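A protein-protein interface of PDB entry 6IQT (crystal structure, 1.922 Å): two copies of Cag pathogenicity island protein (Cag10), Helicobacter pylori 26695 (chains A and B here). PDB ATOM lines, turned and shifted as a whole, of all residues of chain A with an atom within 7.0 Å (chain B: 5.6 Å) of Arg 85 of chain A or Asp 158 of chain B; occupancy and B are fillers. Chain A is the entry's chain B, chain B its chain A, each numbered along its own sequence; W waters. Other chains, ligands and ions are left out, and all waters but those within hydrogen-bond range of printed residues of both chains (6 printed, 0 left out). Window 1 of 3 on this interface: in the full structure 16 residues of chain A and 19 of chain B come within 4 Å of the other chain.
Water W5 lies within hydrogen-bond range of the side-chain amide oxygen (OE1) of Gln 160 of chain B (2.4 Å), the backbone carbonyl oxygen (O) of Ala 86 of chain A (3.2 Å) and the guanidinium group (NH2) of Arg 53 of chain A (3.2 Å).
Water W2 lies within hydrogen-bond range of NE of Arg 85 of chain A, OE1 of Glu 87 of chain A and NE2 of Gln 68 of chain B.
Water W3 lies within hydrogen-bond range of the side-chain carboxylate of Asp 118 of chain A (2.8 Å), the backbone NH of Gln 68 of chain B (2.9 Å) and the backbone carbonyl oxygen of Phe 65 of chain B (3.4 Å).
Water W6 lies within hydrogen-bond range of the side-chain carboxylate of Asp 118 of chain A (3.0 Å) and the side-chain amide oxygen of Gln 68 of chain B (3.0 Å).
Water W1 lies within hydrogen-bond range of the backbone carbonyl oxygen of Ile 159 of chain B and the guanidinium group of Arg 85 of chain A.
Water W4 lies within hydrogen-bond range of the side-chain amide nitrogen of Gln 160 of chain B, the backbone carbonyl oxygen of Ala 86 of chain A, the backbone carbonyl oxygen of Tyr 45 of chain A and the guanidinium group of Arg 85 of chain A.
Printed residues of chain B within 4 Å of Ser 46 of chain A: Asp 158 and Gln 160.
Of the printed residues of chain B, Asn 48 of chain A touches Phe 157 (2.9 Å) and Asp 158 (3.7 Å).
Of chain B, only Gln 68, Asp 158, Ile 159 and Gln 160 come within 4 Å of Arg 85 of chain A.
Of the printed residues of chain A, Gln 68 of chain B touches Arg 85.
Printed residues of chain A within 4 Å of Tyr 134 of chain B: Ser 49 (3.6 Å).
Of the printed residues of chain A, Phe 157 of chain B touches Asn 48.
Asp 158 of chain B touches just these residues of chain A: Ser 46 (2.5 Å), Asn 48 (3.7 Å), Ser 49 (2.8 Å) and Arg 85 (3.0 Å).
The nearest residue of chain B that does not touch Arg 85 of chain A is Phe 65 of chain B (4.4 Å).
Ser 46 of chain A touches Gln 160 of chain B (CB to NE2, 3.7 Å).
Asp 158 of chain B touches Asn 48 of chain A.
CB of Ser 49 of chain A touches CE1 of Tyr 134 of chain B, 3.6 Å away.
Arg 85 of chain A touches Gln 68 of chain B (CD to OE1, 3.3 Å).
O of Ile 159 of chain B touches NH2 of Arg 85 of chain A, at 3.6 Å.
Arg 85 of chain A touches Gln 160 of chain B.
Along chain A the printed residues that touch a printed residue of chain B span positions 46 to 85.
Printed residues of chain B that touch a printed residue of chain A: Gln 68, Tyr 134, Phe 157, Asp 158, Ile 159 and Gln 160.
Among the printed residues, 11 pairs touch across the chains.
No position is printed for both chains.
Of the 11 pairs that touch across the chains among the printed residues, none has its exchanged pair printed and touching as well.
The side-chain carboxylate of Asp 158 of chain B lies within hydrogen-bond range of the side-chain hydroxyl of Ser 46 of chain A (2.5 Å).
The side-chain amide nitrogen (ND2) of Asn 48 of chain A lies within hydrogen-bond range of the backbone carbonyl oxygen (O) of Phe 157 of chain B (2.9 Å).
The guanidinium group of Arg 85 of chain A lies within salt-bridge range of the side-chain carboxylate of Asp 158 of chain B, at 3.0 Å.
The side-chain hydroxyl of Ser 49 of chain A lies within hydrogen-bond range of the side-chain carboxylate of Asp 158 of chain B (2.8 Å).
The side-chain amide nitrogen of Gln 160 of chain B lies close to the guanidinium group of Arg 53 of chain A.
The backbone carbonyl oxygen (O) of Asp 158 of chain B is in hydrogen-bond range of the backbone NH (N) of Tyr 134 of chain B (3.0 Å).
N of Thr 132 of chain B sits at hydrogen-bond distance from O of Gln 160 of chain B, at 2.9 Å.
OG of Ser 46 of chain A sits at hydrogen-bond distance from NH1 of Arg 85 of chain A (3.1 Å).
O of Tyr 134 of chain B lies within hydrogen-bond range of N of Phe 157 of chain B, 2.7 Å away.
N of Thr 116 of chain A lies within hydrogen-bond range of O of Arg 85 of chain A (2.9 Å).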
ATOM      1  N   GLY A  44     -18.951  13.563  11.999  1.00  0.00           N
ATOM      2  CA  GLY A  44     -18.568  13.205  10.650  1.00  0.00           C
ATOM      3  C   GLY A  44     -17.781  11.898  10.626  1.00  0.00           C
ATOM      4  O   GLY A  44     -17.515  11.284  11.653  1.00  0.00           O
ATOM      5  N   TYR A  45     -17.426  11.464   9.417  1.00  0.00           N
ATOM      6  CA  TYR A  45     -16.710  10.196   9.267  1.00  0.00           C
ATOM      7  C   TYR A  45     -16.003  10.139   7.926  1.00  0.00           C
ATOM      8  O   TYR A  45     -16.578  10.487   6.890  1.00  0.00           O
ATOM      9  CB  TYR A  45     -17.655   8.976   9.395  1.00  0.00           C
ATOM     10  CG  TYR A  45     -16.935   7.652   9.181  1.00  0.00           C
ATOM     11  CD1 TYR A  45     -16.338   6.986  10.242  1.00  0.00           C
ATOM     12  CD2 TYR A  45     -16.830   7.087   7.905  1.00  0.00           C
ATOM     13  CE1 TYR A  45     -15.668   5.791  10.056  1.00  0.00           C
ATOM     14  CE2 TYR A  45     -16.147   5.886   7.707  1.00  0.00           C
ATOM     15  CZ  TYR A  45     -15.575   5.249   8.793  1.00  0.00           C
ATOM     16  OH  TYR A  45     -14.897   4.064   8.615  1.00  0.00           O
ATOM     17  N   SER A  46     -14.761   9.657   7.951  1.00  0.00           N
ATOM     18  CA  SER A  46     -14.025   9.341   6.735  1.00  0.00           C
ATOM     19  C   SER A  46     -13.030   8.246   7.093  1.00  0.00           C
ATOM     20  O   SER A  46     -12.338   8.365   8.104  1.00  0.00           O
ATOM     21  CB  SER A  46     -13.290  10.588   6.192  1.00  0.00           C
ATOM     22  OG  SER A  46     -12.662  10.286   4.973  1.00  0.00           O
ATOM     23  N   LYS A  47     -12.940   7.203   6.268  1.00  0.00           N
ATOM     24  CA  LYS A  47     -12.099   6.065   6.627  1.00  0.00           C
ATOM     25  C   LYS A  47     -10.627   6.463   6.739  1.00  0.00           C
ATOM     26  O   LYS A  47      -9.974   6.173   7.746  1.00  0.00           O
ATOM     27  CB  LYS A  47     -12.291   4.935   5.605  1.00  0.00           C
ATOM     28  CG  LYS A  47     -11.419   3.702   5.833  1.00  0.00           C
ATOM     29  CD  LYS A  47     -11.459   3.212   7.279  1.00  0.00           C
ATOM     30  CE  LYS A  47     -10.631   1.933   7.454  1.00  0.00           C
ATOM     31  NZ  LYS A  47     -11.260   0.741   6.800  1.00  0.00           N
ATOM     32  N   ASN A  48     -10.094   7.164   5.733  1.00  0.00           N
ATOM     33  CA  ASN A  48      -8.642   7.297   5.618  1.00  0.00           C
ATOM     34  C   ASN A  48      -8.008   8.133   6.733  1.00  0.00           C
ATOM     35  O   ASN A  48      -6.812   7.974   7.008  1.00  0.00           O
ATOM     36  CB  ASN A  48      -8.288   7.900   4.263  1.00  0.00           C
ATOM     37  CG  ASN A  48      -8.261   6.866   3.167  1.00  0.00           C
ATOM     38  OD1 ASN A  48      -8.122   5.679   3.441  1.00  0.00           O
ATOM     39  ND2 ASN A  48      -8.406   7.307   1.921  1.00  0.00           N
ATOM     40  N   SER A  49      -8.754   9.045   7.360  1.00  0.00           N
ATOM     41  CA  SER A  49      -8.176   9.900   8.391  1.00  0.00           C
ATOM     42  C   SER A  49      -8.748   9.625   9.779  1.00  0.00           C
ATOM     43  O   SER A  49      -8.684  10.501  10.650  1.00  0.00           O
ATOM     44  CB  SER A  49      -8.366  11.377   8.022  1.00  0.00           C
ATOM     45  OG  SER A  49      -9.736  11.671   7.759  1.00  0.00           O
ATOM     46  N   LEU A  50      -9.270   8.417  10.017  1.00  0.00           N
ATOM     47  CA  LEU A  50     -10.062   8.164  11.220  1.00  0.00           C
ATOM     48  C   LEU A  50      -9.266   8.396  12.499  1.00  0.00           C
ATOM     49  O   LEU A  50      -9.778   9.003  13.448  1.00  0.00           O
ATOM     50  CB  LEU A  50     -10.627   6.746  11.181  1.00  0.00           C
ATOM     51  CG  LEU A  50     -11.699   6.391  12.213  1.00  0.00           C
ATOM     52  CD1 LEU A  50     -12.776   7.470  12.275  1.00  0.00           C
ATOM     53  CD2 LEU A  50     -12.302   5.023  11.890  1.00  0.00           C
ATOM     54  N   ARG A  53      -8.786  12.134  13.084  1.00  0.00           N
ATOM     55  CA  ARG A  53     -10.055  12.713  13.527  1.00  0.00           C
ATOM     56  C   ARG A  53     -10.243  12.506  15.020  1.00  0.00           C
ATOM     57  O   ARG A  53     -10.600  13.436  15.754  1.00  0.00           O
ATOM     58  CB  ARG A  53     -11.217  12.101  12.742  1.00  0.00           C
ATOM     59  CG  ARG A  53     -12.629  12.514  13.224  1.00  0.00           C
ATOM     60  CD  ARG A  53     -13.731  11.799  12.422  1.00  0.00           C
ATOM     61  NE  ARG A  53     -13.588  12.028  10.980  1.00  0.00           N
ATOM     62  CZ  ARG A  53     -14.235  12.963  10.296  1.00  0.00           C
ATOM     63  NH1 ARG A  53     -15.082  13.787  10.906  1.00  0.00           N
ATOM     64  NH2 ARG A  53     -14.015  13.099   8.996  1.00  0.00           N
ATOM     65  N   PHE A  80     -21.161   3.355  10.068  1.00  0.00           N
ATOM     66  CA  PHE A  80     -20.255   3.526   8.932  1.00  0.00           C
ATOM     67  C   PHE A  80     -19.331   2.319   8.765  1.00  0.00           C
ATOM     68  O   PHE A  80     -18.371   2.165   9.521  1.00  0.00           O
ATOM     69  CB  PHE A  80     -19.462   4.825   9.109  1.00  0.00           C
ATOM     70  CG  PHE A  80     -20.337   6.006   9.434  1.00  0.00           C
ATOM     71  CD1 PHE A  80     -21.429   6.305   8.639  1.00  0.00           C
ATOM     72  CD2 PHE A  80     -20.092   6.793  10.545  1.00  0.00           C
ATOM     73  CE1 PHE A  80     -22.254   7.374   8.935  1.00  0.00           C
ATOM     74  CE2 PHE A  80     -20.897   7.856  10.842  1.00  0.00           C
ATOM     75  CZ  PHE A  80     -21.989   8.151  10.038  1.00  0.00           C
ATOM     76  N   ASP A  82     -17.083   0.262   5.574  1.00  0.00           N
ATOM     77  CA  ASP A  82     -16.557   0.218   4.199  1.00  0.00           C
ATOM     78  C   ASP A  82     -16.710   1.606   3.566  1.00  0.00           C
ATOM     79  O   ASP A  82     -16.262   2.605   4.154  1.00  0.00           O
ATOM     80  CB  ASP A  82     -17.245  -0.916   3.430  1.00  0.00           C
ATOM     81  CG  ASP A  82     -16.576  -2.274   3.626  1.00  0.00           C
ATOM     82  OD1 ASP A  82     -15.524  -2.348   4.294  1.00  0.00           O
ATOM     83  OD2 ASP A  82     -17.120  -3.280   3.110  1.00  0.00           O
ATOM     84  N   LYS A  83     -17.354   1.714   2.399  1.00  0.00           N
ATOM     85  CA  LYS A  83     -17.258   2.878   1.517  1.00  0.00           C
ATOM     86  C   LYS A  83     -18.379   3.864   1.852  1.00  0.00           C
ATOM     87  O   LYS A  83     -19.356   4.012   1.126  1.00  0.00           O
ATOM     88  CB  LYS A  83     -17.353   2.431   0.062  1.00  0.00           C
ATOM     89  CG  LYS A  83     -16.067   1.855  -0.532  1.00  0.00           C
ATOM     90  CD  LYS A  83     -16.172   1.876  -2.046  1.00  0.00           C
ATOM     91  CE  LYS A  83     -15.086   2.722  -2.706  1.00  0.00           C
ATOM     92  NZ  LYS A  83     -15.226   2.725  -4.204  1.00  0.00           N
ATOM     93  N   VAL A  84     -18.225   4.573   2.961  1.00  0.00           N
ATOM     94  CA  VAL A  84     -19.207   5.574   3.370  1.00  0.00           C
ATOM     95  C   VAL A  84     -18.481   6.779   3.965  1.00  0.00           C
ATOM     96  O   VAL A  84     -17.448   6.634   4.629  1.00  0.00           O
ATOM     97  CB  VAL A  84     -20.217   4.970   4.372  1.00  0.00           C
ATOM     98  CG1 VAL A  84     -19.519   4.361   5.561  1.00  0.00           C
ATOM     99  CG2 VAL A  84     -21.220   6.001   4.821  1.00  0.00           C
ATOM    100  N   ARG A  85     -19.016   7.975   3.700  1.00  0.00           N
ATOM    101  CA  ARG A  85     -18.556   9.208   4.322  1.00  0.00           C
ATOM    102  C   ARG A  85     -19.726   9.907   4.998  1.00  0.00           C
ATOM    103  O   ARG A  85     -20.873   9.775   4.568  1.00  0.00           O
ATOM    104  CB  ARG A  85     -17.922  10.159   3.296  1.00  0.00           C
ATOM    105  CG  ARG A  85     -16.817   9.532   2.492  1.00  0.00           C
ATOM    106  CD  ARG A  85     -16.233  10.522   1.491  1.00  0.00           C
ATOM    107  NE  ARG A  85     -15.650  11.674   2.164  1.00  0.00           N
ATOM    108  CZ  ARG A  85     -14.350  11.806   2.427  1.00  0.00           C
ATOM    109  NH1 ARG A  85     -13.487  10.855   2.062  1.00  0.00           N
ATOM    110  NH2 ARG A  85     -13.918  12.895   3.040  1.00  0.00           N
ATOM    111  N   ALA A  86     -19.424  10.666   6.057  1.00  0.00           N
ATOM    112  CA  ALA A  86     -20.413  11.524   6.700  1.00  0.00           C
ATOM    113  C   ALA A  86     -19.838  12.915   6.932  1.00  0.00           C
ATOM    114  O   ALA A  86     -18.686  13.065   7.360  1.00  0.00           O
ATOM    115  CB  ALA A  86     -20.899  10.938   8.027  1.00  0.00           C
ATOM    116  N   GLU A  87     -20.655  13.932   6.656  1.00  0.00           N
ATOM    117  CA  GLU A  87     -20.310  15.322   6.929  1.00  0.00           C
ATOM    118  C   GLU A  87     -21.388  15.927   7.821  1.00  0.00           C
ATOM    119  O   GLU A  87     -22.587  15.705   7.609  1.00  0.00           O
ATOM    120  CB  GLU A  87     -20.174  16.134   5.629  1.00  0.00           C
ATOM    121  CG  GLU A  87     -19.011  15.709   4.745  1.00  0.00           C
ATOM    122  CD  GLU A  87     -19.356  15.734   3.259  1.00  0.00           C
ATOM    123  OE1 GLU A  87     -19.264  14.667   2.606  1.00  0.00           O
ATOM    124  OE2 GLU A  87     -19.718  16.819   2.742  1.00  0.00           O
ATOM    125  N   ILE A 113     -26.473  15.938   9.457  1.00  0.00           N
ATOM    126  CA  ILE A 113     -25.474  14.939   9.096  1.00  0.00           C
ATOM    127  C   ILE A 113     -25.858  14.366   7.740  1.00  0.00           C
ATOM    128  O   ILE A 113     -26.957  13.818   7.579  1.00  0.00           O
ATOM    129  CB  ILE A 113     -25.382  13.838  10.159  1.00  0.00           C
ATOM    130  CG1 ILE A 113     -25.015  14.438  11.524  1.00  0.00           C
ATOM    131  CG2 ILE A 113     -24.382  12.735   9.730  1.00  0.00           C
ATOM    132  CD1 ILE A 113     -25.260  13.461  12.688  1.00  0.00           C
ATOM    133  N   LYS A 114     -24.966  14.481   6.759  1.00  0.00           N
ATOM    134  CA  LYS A 114     -25.219  13.907   5.440  1.00  0.00           C
ATOM    135  C   LYS A 114     -24.329  12.687   5.246  1.00  0.00           C
ATOM    136  O   LYS A 114     -23.096  12.771   5.383  1.00  0.00           O
ATOM    137  CB  LYS A 114     -25.001  14.929   4.331  1.00  0.00           C
ATOM    138  CG  LYS A 114     -25.215  14.356   2.937  1.00  0.00           C
ATOM    139  CD  LYS A 114     -24.952  15.425   1.885  1.00  0.00           C
ATOM    140  CE  LYS A 114     -23.470  15.701   1.759  1.00  0.00           C
ATOM    141  NZ  LYS A 114     -23.201  16.620   0.623  1.00  0.00           N
ATOM    142  N   ILE A 115     -24.960  11.551   4.959  1.00  0.00           N
ATOM    143  CA  ILE A 115     -24.282  10.264   4.849  1.00  0.00           C
ATOM    144  C   ILE A 115     -24.300   9.848   3.383  1.00  0.00           C
ATOM    145  O   ILE A 115     -25.375   9.653   2.803  1.00  0.00           O
ATOM    146  CB  ILE A 115     -24.949   9.207   5.739  1.00  0.00           C
ATOM    147  CG1 ILE A 115     -24.890   9.652   7.222  1.00  0.00           C
ATOM    148  CG2 ILE A 115     -24.290   7.838   5.523  1.00  0.00           C
ATOM    149  CD1 ILE A 115     -25.822   8.881   8.143  1.00  0.00           C
ATOM    150  N   THR A 116     -23.112   9.693   2.783  1.00  0.00           N
ATOM    151  CA  THR A 116     -23.041   9.408   1.356  1.00  0.00           C
ATOM    152  C   THR A 116     -22.207   8.162   1.101  1.00  0.00           C
ATOM    153  O   THR A 116     -21.181   7.955   1.764  1.00  0.00           O
ATOM    154  CB  THR A 116     -22.427  10.586   0.588  1.00  0.00           C
ATOM    155  OG1 THR A 116     -21.078  10.768   1.018  1.00  0.00           O
ATOM    156  CG2 THR A 116     -23.197  11.868   0.859  1.00  0.00           C
ATOM    157  N   PRO A 117     -22.622   7.304   0.171  1.00  0.00           N
ATOM    158  CA  PRO A 117     -21.754   6.192  -0.218  1.00  0.00           C
ATOM    159  C   PRO A 117     -20.475   6.763  -0.808  1.00  0.00           C
ATOM    160  O   PRO A 117     -20.493   7.778  -1.516  1.00  0.00           O
ATOM    161  CB  PRO A 117     -22.583   5.434  -1.264  1.00  0.00           C
ATOM    162  CG  PRO A 117     -23.491   6.456  -1.824  1.00  0.00           C
ATOM    163  CD  PRO A 117     -23.797   7.423  -0.710  1.00  0.00           C
ATOM    164  N   ASP A 118     -19.356   6.161  -0.451  1.00  0.00           N
ATOM    165  CA  ASP A 118     -18.081   6.599  -1.022  1.00  0.00           C
ATOM    166  C   ASP A 118     -17.876   5.908  -2.367  1.00  0.00           C
ATOM    167  O   ASP A 118     -16.848   5.294  -2.642  1.00  0.00           O
ATOM    168  CB  ASP A 118     -16.933   6.326  -0.051  1.00  0.00           C
ATOM    169  CG  ASP A 118     -15.632   7.077  -0.421  1.00  0.00           C
ATOM    170  OD1 ASP A 118     -15.680   8.263  -0.840  1.00  0.00           O
ATOM    171  OD2 ASP A 118     -14.548   6.475  -0.271  1.00  0.00           O
ATOM    172  N   PHE B  65      -9.464   8.072  -2.800  1.00  0.00           N
ATOM    173  CA  PHE B  65     -10.049   9.397  -2.672  1.00  0.00           C
ATOM    174  C   PHE B  65     -10.681   9.911  -3.965  1.00  0.00           C
ATOM    175  O   PHE B  65     -11.334  10.962  -3.943  1.00  0.00           O
ATOM    176  CB  PHE B  65      -8.963  10.382  -2.177  1.00  0.00           C
ATOM    177  CG  PHE B  65      -9.469  11.771  -1.914  1.00  0.00           C
ATOM    178  CD1 PHE B  65     -10.356  12.016  -0.871  1.00  0.00           C
ATOM    179  CD2 PHE B  65      -9.080  12.828  -2.728  1.00  0.00           C
ATOM    180  CE1 PHE B  65     -10.841  13.295  -0.630  1.00  0.00           C
ATOM    181  CE2 PHE B  65      -9.560  14.106  -2.499  1.00  0.00           C
ATOM    182  CZ  PHE B  65     -10.441  14.342  -1.446  1.00  0.00           C
ATOM    183  N   GLN B  68     -14.536  10.876  -4.037  1.00  0.00           N
ATOM    184  CA  GLN B  68     -14.914  12.103  -3.346  1.00  0.00           C
ATOM    185  C   GLN B  68     -14.464  13.345  -4.116  1.00  0.00           C
ATOM    186  O   GLN B  68     -15.199  14.341  -4.190  1.00  0.00           O
ATOM    187  CB  GLN B  68     -14.336  12.079  -1.928  1.00  0.00           C
ATOM    188  CG  GLN B  68     -14.589  13.339  -1.131  1.00  0.00           C
ATOM    189  CD  GLN B  68     -16.054  13.572  -0.851  1.00  0.00           C
ATOM    190  OE1 GLN B  68     -16.888  12.670  -0.994  1.00  0.00           O
ATOM    191  NE2 GLN B  68     -16.382  14.790  -0.461  1.00  0.00           N
ATOM    192  N   THR B 132      -8.235  20.991   5.378  1.00  0.00           N
ATOM    193  CA  THR B 132      -7.279  20.005   5.866  1.00  0.00           C
ATOM    194  C   THR B 132      -7.109  18.928   4.804  1.00  0.00           C
ATOM    195  O   THR B 132      -8.097  18.340   4.357  1.00  0.00           O
ATOM    196  CB  THR B 132      -7.795  19.354   7.156  1.00  0.00           C
ATOM    197  OG1 THR B 132      -8.087  20.360   8.130  1.00  0.00           O
ATOM    198  CG2 THR B 132      -6.791  18.359   7.703  1.00  0.00           C
ATOM    199  N   ILE B 133      -5.877  18.638   4.403  1.00  0.00           N
ATOM    200  CA  ILE B 133      -5.693  17.515   3.490  1.00  0.00           C
ATOM    201  C   ILE B 133      -4.700  16.536   4.103  1.00  0.00           C
ATOM    202  O   ILE B 133      -3.792  16.907   4.853  1.00  0.00           O
ATOM    203  CB  ILE B 133      -5.239  17.911   2.059  1.00  0.00           C
ATOM    204  CG1 ILE B 133      -3.783  18.339   2.038  1.00  0.00           C
ATOM    205  CG2 ILE B 133      -6.162  18.961   1.387  1.00  0.00           C
ATOM    206  CD1 ILE B 133      -3.094  17.972   0.742  1.00  0.00           C
ATOM    207  N   TYR B 134      -4.875  15.266   3.760  1.00  0.00           N
ATOM    208  CA  TYR B 134      -3.969  14.204   4.167  1.00  0.00           C
ATOM    209  C   TYR B 134      -3.306  13.657   2.914  1.00  0.00           C
ATOM    210  O   TYR B 134      -3.996  13.344   1.939  1.00  0.00           O
ATOM    211  CB  TYR B 134      -4.732  13.103   4.907  1.00  0.00           C
ATOM    212  CG  TYR B 134      -5.410  13.581   6.176  1.00  0.00           C
ATOM    213  CD1 TYR B 134      -6.621  14.257   6.140  1.00  0.00           C
ATOM    214  CD2 TYR B 134      -4.828  13.358   7.411  1.00  0.00           C
ATOM    215  CE1 TYR B 134      -7.242  14.696   7.330  1.00  0.00           C
ATOM    216  CE2 TYR B 134      -5.420  13.799   8.575  1.00  0.00           C
ATOM    217  CZ  TYR B 134      -6.625  14.457   8.535  1.00  0.00           C
ATOM    218  OH  TYR B 134      -7.204  14.875   9.721  1.00  0.00           O
ATOM    219  N   VAL B 156      -3.331  12.753  -2.576  1.00  0.00           N
ATOM    220  CA  VAL B 156      -4.248  13.137  -1.504  1.00  0.00           C
ATOM    221  C   VAL B 156      -5.098  11.933  -1.120  1.00  0.00           C
ATOM    222  O   VAL B 156      -5.662  11.256  -1.987  1.00  0.00           O
ATOM    223  CB  VAL B 156      -5.139  14.316  -1.940  1.00  0.00           C
ATOM    224  CG1 VAL B 156      -6.167  14.659  -0.857  1.00  0.00           C
ATOM    225  CG2 VAL B 156      -4.262  15.538  -2.275  1.00  0.00           C
ATOM    226  N   PHE B 157      -5.212  11.675   0.186  1.00  0.00           N
ATOM    227  CA  PHE B 157      -6.002  10.552   0.676  1.00  0.00           C
ATOM    228  C   PHE B 157      -7.296  10.970   1.335  1.00  0.00           C
ATOM    229  O   PHE B 157      -8.209  10.144   1.444  1.00  0.00           O
ATOM    230  CB  PHE B 157      -5.197   9.726   1.687  1.00  0.00           C
ATOM    231  CG  PHE B 157      -4.174   8.841   1.054  1.00  0.00           C
ATOM    232  CD1 PHE B 157      -3.041   9.386   0.451  1.00  0.00           C
ATOM    233  CD2 PHE B 157      -4.332   7.460   1.062  1.00  0.00           C
ATOM    234  CE1 PHE B 157      -2.081   8.561  -0.148  1.00  0.00           C
ATOM    235  CE2 PHE B 157      -3.372   6.629   0.473  1.00  0.00           C
ATOM    236  CZ  PHE B 157      -2.246   7.182  -0.132  1.00  0.00           C
ATOM    237  N   ASP B 158      -7.401  12.218   1.769  1.00  0.00           N
ATOM    238  CA  ASP B 158      -8.600  12.680   2.456  1.00  0.00           C
ATOM    239  C   ASP B 158      -8.574  14.193   2.516  1.00  0.00           C
ATOM    240  O   ASP B 158      -7.515  14.819   2.383  1.00  0.00           O
ATOM    241  CB  ASP B 158      -8.686  12.099   3.868  1.00  0.00           C
ATOM    242  CG  ASP B 158     -10.121  11.770   4.279  1.00  0.00           C
ATOM    243  OD1 ASP B 158     -11.068  12.364   3.706  1.00  0.00           O
ATOM    244  OD2 ASP B 158     -10.293  10.907   5.172  1.00  0.00           O
ATOM    245  N   ILE B 159      -9.751  14.777   2.756  1.00  0.00           N
ATOM    246  CA  ILE B 159      -9.881  16.218   2.899  1.00  0.00           C
ATOM    247  C   ILE B 159     -11.006  16.488   3.888  1.00  0.00           C
ATOM    248  O   ILE B 159     -11.962  15.714   4.000  1.00  0.00           O
ATOM    249  CB  ILE B 159     -10.137  16.911   1.537  1.00  0.00           C
ATOM    250  CG1 ILE B 159      -9.937  18.424   1.641  1.00  0.00           C
ATOM    251  CG2 ILE B 159     -11.541  16.607   1.004  1.00  0.00           C
ATOM    252  CD1 ILE B 159     -10.038  19.139   0.282  1.00  0.00           C
ATOM    253  N   GLN B 160     -10.877  17.585   4.623  1.00  0.00           N
ATOM    254  CA  GLN B 160     -11.931  18.055   5.522  1.00  0.00           C
ATOM    255  C   GLN B 160     -12.010  19.561   5.344  1.00  0.00           C
ATOM    256  O   GLN B 160     -10.977  20.222   5.202  1.00  0.00           O
ATOM    257  CB  GLN B 160     -11.648  17.693   6.989  1.00  0.00           C
ATOM    258  CG  GLN B 160     -11.679  16.182   7.294  1.00  0.00           C
ATOM    259  CD  GLN B 160     -13.028  15.520   6.954  1.00  0.00           C
ATOM    260  OE1 GLN B 160     -14.098  16.086   7.207  1.00  0.00           O
ATOM    261  NE2 GLN B 160     -12.974  14.315   6.377  1.00  0.00           N
HETATM  262  O   HOH W   1     -14.797  15.940   3.026  1.00  0.00           O
HETATM  263  O   HOH W   2     -16.508  13.960   2.929  1.00  0.00           O
HETATM  264  O   HOH W   3     -13.442   8.669  -2.521  1.00  0.00           O
HETATM  265  O   HOH W   4     -15.982  13.425   5.565  1.00  0.00           O
HETATM  266  O   HOH W   5     -16.219  15.046   7.734  1.00  0.00           O
HETATM  267  O   HOH W   6     -17.579  10.035  -2.319  1.00  0.00           O
